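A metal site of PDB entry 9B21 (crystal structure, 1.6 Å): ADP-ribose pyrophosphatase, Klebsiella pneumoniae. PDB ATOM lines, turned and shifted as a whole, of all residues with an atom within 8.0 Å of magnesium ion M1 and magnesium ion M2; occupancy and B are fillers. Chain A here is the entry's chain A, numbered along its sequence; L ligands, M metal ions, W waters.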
ATOM      1  N   ALA A  68      26.744  -3.101  10.651  1.00  0.00           N
ATOM      2  CA  ALA A  68      25.303  -3.121  10.691  1.00  0.00           C
ATOM      3  C   ALA A  68      24.806  -4.026   9.573  1.00  0.00           C
ATOM      4  O   ALA A  68      25.369  -4.018   8.471  1.00  0.00           O
ATOM      5  CB  ALA A  68      24.736  -1.709  10.553  1.00  0.00           C
ATOM      6  N   VAL A  83      21.324 -10.121  -1.387  1.00  0.00           N
ATOM      7  CA  VAL A  83      22.315  -9.502  -2.272  1.00  0.00           C
ATOM      8  C   VAL A  83      23.432 -10.496  -2.507  1.00  0.00           C
ATOM      9  O   VAL A  83      23.875 -11.189  -1.583  1.00  0.00           O
ATOM     10  CB  VAL A  83      22.895  -8.177  -1.724  1.00  0.00           C
ATOM     11  CG1 VAL A  83      21.833  -7.091  -1.761  1.00  0.00           C
ATOM     12  CG2 VAL A  83      23.419  -8.336  -0.331  1.00  0.00           C
ATOM     13  N   GLN A  85      27.306 -11.096  -3.894  1.00  0.00           N
ATOM     14  CA  GLN A  85      28.589 -10.493  -4.250  1.00  0.00           C
ATOM     15  C   GLN A  85      29.685 -11.494  -3.943  1.00  0.00           C
ATOM     16  O   GLN A  85      29.492 -12.441  -3.167  1.00  0.00           O
ATOM     17  CB  GLN A  85      28.809  -9.182  -3.491  1.00  0.00           C
ATOM     18  CG  GLN A  85      28.951  -9.389  -2.014  1.00  0.00           C
ATOM     19  CD  GLN A  85      28.608  -8.143  -1.197  1.00  0.00           C
ATOM     20  OE1 GLN A  85      27.648  -8.127  -0.414  1.00  0.00           O
ATOM     21  NE2 GLN A  85      29.389  -7.106  -1.375  1.00  0.00           N
ATOM     22  N   ARG A  87      32.899 -12.897  -2.199  1.00  0.00           N
ATOM     23  CA  ARG A  87      33.619 -12.802  -0.922  1.00  0.00           C
ATOM     24  C   ARG A  87      34.816 -13.732  -1.055  1.00  0.00           C
ATOM     25  O   ARG A  87      34.688 -14.950  -0.914  1.00  0.00           O
ATOM     26  CB  ARG A  87      32.735 -13.208   0.231  1.00  0.00           C
ATOM     27  CG  ARG A  87      31.528 -12.330   0.421  1.00  0.00           C
ATOM     28  CD  ARG A  87      31.948 -10.958   0.850  1.00  0.00           C
ATOM     29  NE  ARG A  87      30.786 -10.203   1.305  1.00  0.00           N
ATOM     30  CZ  ARG A  87      30.815  -8.961   1.754  1.00  0.00           C
ATOM     31  NH1 ARG A  87      31.931  -8.236   1.742  1.00  0.00           N
ATOM     32  NH2 ARG A  87      29.697  -8.435   2.264  1.00  0.00           N
ATOM     33  N   GLU A 101      23.624 -12.936   0.592  1.00  0.00           N
ATOM     34  CA  GLU A 101      23.850 -12.278   1.880  1.00  0.00           C
ATOM     35  C   GLU A 101      22.780 -11.247   2.188  1.00  0.00           C
ATOM     36  O   GLU A 101      21.949 -10.882   1.368  1.00  0.00           O
ATOM     37  CB  GLU A 101      25.186 -11.521   1.888  1.00  0.00           C
ATOM     38  CG  GLU A 101      26.395 -12.322   1.612  1.00  0.00           C
ATOM     39  CD  GLU A 101      27.652 -11.462   1.680  1.00  0.00           C
ATOM     40  OE1 GLU A 101      27.558 -10.240   1.484  1.00  0.00           O
ATOM     41  OE2 GLU A 101      28.732 -11.992   1.995  1.00  0.00           O
ATOM     42  N   MET A 102      22.869 -10.757   3.420  1.00  0.00           N
ATOM     43  CA  MET A 102      22.146  -9.579   3.862  1.00  0.00           C
ATOM     44  C   MET A 102      22.877  -8.310   3.451  1.00  0.00           C
ATOM     45  O   MET A 102      24.092  -8.288   3.278  1.00  0.00           O
ATOM     46  CB  MET A 102      22.017  -9.574   5.397  1.00  0.00           C
ATOM     47  CG  MET A 102      21.545 -10.837   5.988  1.00  0.00           C
ATOM     48  SD  MET A 102      19.766 -11.126   5.837  1.00  0.00           S
ATOM     49  CE  MET A 102      19.587 -12.264   4.494  1.00  0.00           C
ATOM     50  N   VAL A 103      22.096  -7.250   3.295  1.00  0.00           N
ATOM     51  CA  VAL A 103      22.633  -5.896   3.196  1.00  0.00           C
ATOM     52  C   VAL A 103      23.469  -5.635   4.432  1.00  0.00           C
ATOM     53  O   VAL A 103      23.056  -5.977   5.550  1.00  0.00           O
ATOM     54  CB  VAL A 103      21.451  -4.908   3.086  1.00  0.00           C
ATOM     55  CG1 VAL A 103      21.878  -3.481   3.258  1.00  0.00           C
ATOM     56  CG2 VAL A 103      20.719  -5.140   1.775  1.00  0.00           C
ATOM     57  N   ALA A 104      24.664  -5.088   4.270  1.00  0.00           N
ATOM     58  CA  ALA A 104      25.516  -4.928   5.447  1.00  0.00           C
ATOM     59  C   ALA A 104      26.639  -3.961   5.114  1.00  0.00           C
ATOM     60  O   ALA A 104      27.107  -3.900   3.983  1.00  0.00           O
ATOM     61  CB  ALA A 104      26.096  -6.265   5.922  1.00  0.00           C
ATOM     62  N   GLY A 105      27.075  -3.225   6.136  1.00  0.00           N
ATOM     63  CA  GLY A 105      28.200  -2.328   5.958  1.00  0.00           C
ATOM     64  C   GLY A 105      28.857  -1.985   7.278  1.00  0.00           C
ATOM     65  O   GLY A 105      28.274  -2.111   8.359  1.00  0.00           O
ATOM     66  N   MET A 106      30.088  -1.521   7.170  1.00  0.00           N
ATOM     67  CA  MET A 106      30.814  -1.132   8.362  1.00  0.00           C
ATOM     68  C   MET A 106      30.237   0.164   8.925  1.00  0.00           C
ATOM     69  O   MET A 106      29.711   1.012   8.185  1.00  0.00           O
ATOM     70  CB  MET A 106      32.305  -1.004   8.042  1.00  0.00           C
ATOM     71  CG  MET A 106      32.924  -2.359   7.664  1.00  0.00           C
ATOM     72  SD  MET A 106      34.707  -2.396   7.351  1.00  0.00           S
ATOM     73  CE  MET A 106      34.802  -1.865   5.639  1.00  0.00           C
ATOM     74  N   VAL A 116      23.286   3.320   9.160  1.00  0.00           N
ATOM     75  CA  VAL A 116      24.112   2.558   8.232  1.00  0.00           C
ATOM     76  C   VAL A 116      23.250   1.564   7.466  1.00  0.00           C
ATOM     77  O   VAL A 116      23.373   1.443   6.236  1.00  0.00           O
ATOM     78  CB  VAL A 116      25.250   1.846   8.985  1.00  0.00           C
ATOM     79  CG1 VAL A 116      25.956   0.819   8.076  1.00  0.00           C
ATOM     80  CG2 VAL A 116      26.232   2.874   9.538  1.00  0.00           C
ATOM     81  N   ARG A 119      21.317   3.346   4.755  1.00  0.00           N
ATOM     82  CA  ARG A 119      22.166   3.783   3.654  1.00  0.00           C
ATOM     83  C   ARG A 119      22.563   2.599   2.786  1.00  0.00           C
ATOM     84  O   ARG A 119      22.525   2.680   1.550  1.00  0.00           O
ATOM     85  CB  ARG A 119      23.429   4.487   4.183  1.00  0.00           C
ATOM     86  CG  ARG A 119      24.336   4.987   3.055  1.00  0.00           C
ATOM     87  CD  ARG A 119      25.685   5.515   3.538  1.00  0.00           C
ATOM     88  NE  ARG A 119      26.508   4.462   4.131  1.00  0.00           N
ATOM     89  CZ  ARG A 119      26.991   4.492   5.370  1.00  0.00           C
ATOM     90  NH1 ARG A 119      26.767   5.504   6.189  1.00  0.00           N
ATOM     91  NH2 ARG A 119      27.752   3.477   5.787  1.00  0.00           N
ATOM     92  N   GLU A 120      22.977   1.504   3.410  1.00  0.00           N
ATOM     93  CA  GLU A 120      23.430   0.361   2.630  1.00  0.00           C
ATOM     94  C   GLU A 120      22.289  -0.305   1.880  1.00  0.00           C
ATOM     95  O   GLU A 120      22.506  -0.865   0.800  1.00  0.00           O
ATOM     96  CB  GLU A 120      24.131  -0.663   3.531  1.00  0.00           C
ATOM     97  CG  GLU A 120      25.417  -0.165   4.181  1.00  0.00           C
ATOM     98  CD  GLU A 120      26.638  -0.194   3.287  1.00  0.00           C
ATOM     99  OE1 GLU A 120      26.533  -0.660   2.145  1.00  0.00           O
ATOM    100  OE2 GLU A 120      27.705   0.241   3.742  1.00  0.00           O
ATOM    101  N   ALA A 121      21.068  -0.258   2.415  1.00  0.00           N
ATOM    102  CA  ALA A 121      19.959  -0.848   1.677  1.00  0.00           C
ATOM    103  C   ALA A 121      19.802  -0.173   0.328  1.00  0.00           C
ATOM    104  O   ALA A 121      19.527  -0.830  -0.678  1.00  0.00           O
ATOM    105  CB  ALA A 121      18.671  -0.751   2.491  1.00  0.00           C
ATOM    106  N   GLU A 123      22.292   1.630  -1.297  1.00  0.00           N
ATOM    107  CA  GLU A 123      23.498   1.492  -2.097  1.00  0.00           C
ATOM    108  C   GLU A 123      23.615   0.093  -2.677  1.00  0.00           C
ATOM    109  O   GLU A 123      24.085  -0.084  -3.814  1.00  0.00           O
ATOM    110  CB  GLU A 123      24.726   1.802  -1.239  1.00  0.00           C
ATOM    111  CG  GLU A 123      24.860   3.252  -0.820  1.00  0.00           C
ATOM    112  CD  GLU A 123      26.180   3.531  -0.104  1.00  0.00           C
ATOM    113  OE1 GLU A 123      26.880   2.567   0.274  1.00  0.00           O
ATOM    114  OE2 GLU A 123      26.515   4.722   0.051  1.00  0.00           O
ATOM    115  N   GLU A 124      23.241  -0.921  -1.908  1.00  0.00           N
ATOM    116  CA  GLU A 124      23.510  -2.307  -2.264  1.00  0.00           C
ATOM    117  C   GLU A 124      22.342  -2.971  -2.947  1.00  0.00           C
ATOM    118  O   GLU A 124      22.548  -3.936  -3.680  1.00  0.00           O
ATOM    119  CB  GLU A 124      23.898  -3.100  -0.993  1.00  0.00           C
ATOM    120  CG  GLU A 124      25.141  -2.547  -0.319  1.00  0.00           C
ATOM    121  CD  GLU A 124      25.782  -3.508   0.680  1.00  0.00           C
ATOM    122  OE1 GLU A 124      25.118  -4.474   1.119  1.00  0.00           O
ATOM    123  OE2 GLU A 124      26.975  -3.299   0.998  1.00  0.00           O
ATOM    124  N   ALA A 125      21.124  -2.436  -2.800  1.00  0.00           N
ATOM    125  CA  ALA A 125      19.925  -3.087  -3.301  1.00  0.00           C
ATOM    126  C   ALA A 125      18.900  -2.116  -3.880  1.00  0.00           C
ATOM    127  O   ALA A 125      17.847  -2.564  -4.367  1.00  0.00           O
ATOM    128  CB  ALA A 125      19.269  -3.909  -2.163  1.00  0.00           C
ATOM    129  N   GLY A 166      25.718  -1.596  -5.829  1.00  0.00           N
ATOM    130  CA  GLY A 166      27.044  -1.495  -5.276  1.00  0.00           C
ATOM    131  C   GLY A 166      27.796  -0.299  -5.823  1.00  0.00           C
ATOM    132  O   GLY A 166      27.511   0.221  -6.900  1.00  0.00           O
ATOM    133  N   LEU A 167      28.802   0.125  -5.052  1.00  0.00           N
ATOM    134  CA  LEU A 167      29.668   1.232  -5.432  1.00  0.00           C
ATOM    135  C   LEU A 167      30.815   0.724  -6.290  1.00  0.00           C
ATOM    136  O   LEU A 167      31.707   0.013  -5.799  1.00  0.00           O
ATOM    137  CB  LEU A 167      30.217   1.906  -4.169  1.00  0.00           C
ATOM    138  CG  LEU A 167      29.135   2.324  -3.172  1.00  0.00           C
ATOM    139  CD1 LEU A 167      29.704   2.549  -1.776  1.00  0.00           C
ATOM    140  CD2 LEU A 167      28.450   3.587  -3.706  1.00  0.00           C
ATOM    141  N   GLU A 170      34.392   1.531  -5.402  1.00  0.00           N
ATOM    142  CA  GLU A 170      34.900   0.688  -4.325  1.00  0.00           C
ATOM    143  C   GLU A 170      35.010  -0.779  -4.751  1.00  0.00           C
ATOM    144  O   GLU A 170      35.221  -1.646  -3.896  1.00  0.00           O
ATOM    145  CB  GLU A 170      33.998   0.803  -3.094  1.00  0.00           C
ATOM    146  N   GLU A 172      32.718  -2.745  -5.679  1.00  0.00           N
ATOM    147  CA  GLU A 172      31.604  -3.409  -5.006  1.00  0.00           C
ATOM    148  C   GLU A 172      30.539  -3.675  -6.070  1.00  0.00           C
ATOM    149  O   GLU A 172      29.915  -2.743  -6.575  1.00  0.00           O
ATOM    150  CB  GLU A 172      31.073  -2.538  -3.874  1.00  0.00           C
ATOM    151  CG  GLU A 172      30.018  -3.202  -3.004  1.00  0.00           C
ATOM    152  CD  GLU A 172      29.356  -2.222  -2.028  1.00  0.00           C
ATOM    153  OE1 GLU A 172      29.054  -1.072  -2.430  1.00  0.00           O
ATOM    154  OE2 GLU A 172      29.144  -2.604  -0.862  1.00  0.00           O
ATOM    155  N   ILE A 174      27.183  -5.892  -6.942  1.00  0.00           N
ATOM    156  CA  ILE A 174      26.134  -6.565  -6.194  1.00  0.00           C
ATOM    157  C   ILE A 174      24.932  -6.815  -7.080  1.00  0.00           C
ATOM    158  O   ILE A 174      24.478  -5.918  -7.790  1.00  0.00           O
ATOM    159  CB  ILE A 174      25.723  -5.722  -4.973  1.00  0.00           C
ATOM    160  CG1 ILE A 174      26.923  -5.510  -4.044  1.00  0.00           C
ATOM    161  CG2 ILE A 174      24.567  -6.426  -4.228  1.00  0.00           C
ATOM    162  CD1 ILE A 174      26.617  -4.785  -2.746  1.00  0.00           C
HETATM  163  N1  LIG L   1      40.100  -5.910   2.572  1.00  0.00           N
HETATM  164  C1  LIG L   1      40.203  -4.714   1.995  1.00  0.00           C
HETATM  165  N2  LIG L   1      39.245  -3.854   1.692  1.00  0.00           N
HETATM  166  C2  LIG L   1      38.058  -4.357   2.047  1.00  0.00           C
HETATM  167  C3  LIG L   1      37.793  -5.571   2.650  1.00  0.00           C
HETATM  168  C4  LIG L   1      38.891  -6.392   2.914  1.00  0.00           C
HETATM  169  N3  LIG L   1      38.804  -7.600   3.459  1.00  0.00           N
HETATM  170  N4  LIG L   1      36.435  -5.707   2.859  1.00  0.00           N
HETATM  171  C5  LIG L   1      35.918  -4.598   2.402  1.00  0.00           C
HETATM  172  N5  LIG L   1      36.852  -3.738   1.914  1.00  0.00           N
HETATM  173  P1  LIG L   1      31.862  -2.558   3.530  1.00  0.00           P
HETATM  174  P2  LIG L   1      31.428  -5.266   4.218  1.00  0.00           P
HETATM  175  C6  LIG L   1      36.665  -2.457   1.307  1.00  0.00           C
HETATM  176  O1  LIG L   1      31.488  -1.360   4.321  1.00  0.00           O
HETATM  177  O2  LIG L   1      30.049  -5.447   3.732  1.00  0.00           O
HETATM  178  C7  LIG L   1      30.865  -8.894   5.635  1.00  0.00           C
HETATM  179  O3  LIG L   1      30.639 -10.254   5.687  1.00  0.00           O
HETATM  180  C8  LIG L   1      36.124  -2.613  -0.113  1.00  0.00           C
HETATM  181  O4  LIG L   1      36.578  -1.570  -0.945  1.00  0.00           O
HETATM  182  O5  LIG L   1      31.110  -3.022   2.349  1.00  0.00           O
HETATM  183  O6  LIG L   1      32.538  -5.696   3.348  1.00  0.00           O
HETATM  184  C9  LIG L   1      32.083  -8.548   6.491  1.00  0.00           C
HETATM  185  O7  LIG L   1      32.841  -9.643   6.948  1.00  0.00           O
HETATM  186  C10 LIG L   1      34.626  -2.540   0.145  1.00  0.00           C
HETATM  187  O8  LIG L   1      33.906  -2.214  -1.034  1.00  0.00           O
HETATM  188  O9  LIG L   1      31.825  -3.766   4.557  1.00  0.00           O
HETATM  189  C11 LIG L   1      31.507  -7.820   7.706  1.00  0.00           C
HETATM  190  O10 LIG L   1      31.207  -8.725   8.745  1.00  0.00           O
HETATM  191  C12 LIG L   1      34.608  -1.416   1.182  1.00  0.00           C
HETATM  192  O11 LIG L   1      35.726  -1.728   2.042  1.00  0.00           O
HETATM  193  C13 LIG L   1      30.216  -7.221   7.162  1.00  0.00           C
HETATM  194  O12 LIG L   1      29.748  -8.171   6.173  1.00  0.00           O
HETATM  195  C14 LIG L   1      33.377  -1.289   2.026  1.00  0.00           C
HETATM  196  O13 LIG L   1      33.342  -2.366   2.994  1.00  0.00           O
HETATM  197  C15 LIG L   1      30.358  -5.857   6.552  1.00  0.00           C
HETATM  198  O14 LIG L   1      31.524  -5.865   5.689  1.00  0.00           O
HETATM  199 MG    MG M   1      28.099  -1.572   0.879  1.00  0.00          MG
HETATM  200 MG    MG M   2      28.183  -4.733   2.194  1.00  0.00          MG
HETATM  201  O   HOH W   1      28.902  -2.790   2.451  1.00  0.00           O
HETATM  202  O   HOH W   2      27.456  -0.232  -0.534  1.00  0.00           O
HETATM  203  O   HOH W   3      30.018  -0.239   0.795  1.00  0.00           O
HETATM  204  O   HOH W   4      26.786  -6.257   1.772  1.00  0.00           O
HETATM  205  O   HOH W   5      29.381  -4.990   0.260  1.00  0.00           O
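O of Glu 170 sits at hydrogen-bond distance from O8 of the ligand (3.2 Å). The backbone NH (N) of Met 106 is in hydrogen-bond range of an oxygen (O1) of the ligand (3.2 Å). An oxygen (O6) of the ligand lies within salt-bridge range of the guanidinium group (NH1) of Arg 87.
NH2 of Arg 119 lies within salt-bridge range of OE2 of Glu 120 (3.8 Å). The side-chain carboxylate (OE2) of Glu 101 lies within salt-bridge range of the guanidinium group (NE) of Arg 87 (2.8 Å). OE1 of Gln 85 sits at hydrogen-bond distance from NH2 of Arg 87, at 3.4 Å. N of Leu 167 lies within hydrogen-bond range of OE1 of Glu 172 (2.9 Å).
Three residues have an atom within 4 Å of magnesium ion M1: Glu 120, Glu 124 and Glu 172. The nearest printed residue that does not touch magnesium ion M1 is Ala 104 (4.005 Å).
Of the 22 residues printed, 3 come within 4 Å of magnesium ion M2.
Magnesium ion M1 is bound by water W2, at 2.1 Å. OE2 of Glu 124 binds magnesium ion M1 (2.1 Å). Magnesium ion M1 is bound by water W1. OE1 of Glu 120 binds magnesium ion M1, at 2.2 Å. OE2 of Glu 172 is bound to magnesium ion M1 (2.3 Å). Water W3 is bound to magnesium ion M1.
Magnesium ion M2 is bound by water W1, 2.1 Å away. Magnesium ion M2 is bound by water W4 (2.1 Å). OE2 of Glu 124 binds magnesium ion M2 (2.2 Å). O of Ala 104 binds magnesium ion M2, at 2.2 Å. Water W5 is bound to magnesium ion M2. Magnesium ion M2 is bound by O2 of the ligand, 2.5 Å away. Magnesium ion M2 has six donor atoms within binding distance.
Water W2 bridges OE1 of Glu 172 (2.6 Å) and OE1 of Glu 123 (3.0 Å). Water W3 bridges O5 of the ligand (3.4 Å) and OE1 of Glu 172 (3.5 Å). Water W5 lies within hydrogen-bond range of NE2 of Gln 85 (2.7 Å) and O5 of the ligand (3.4 Å). Water W4 lies within hydrogen-bond range of OE1 of Glu 124, OE1 of Gln 85 and N of Ala 104.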
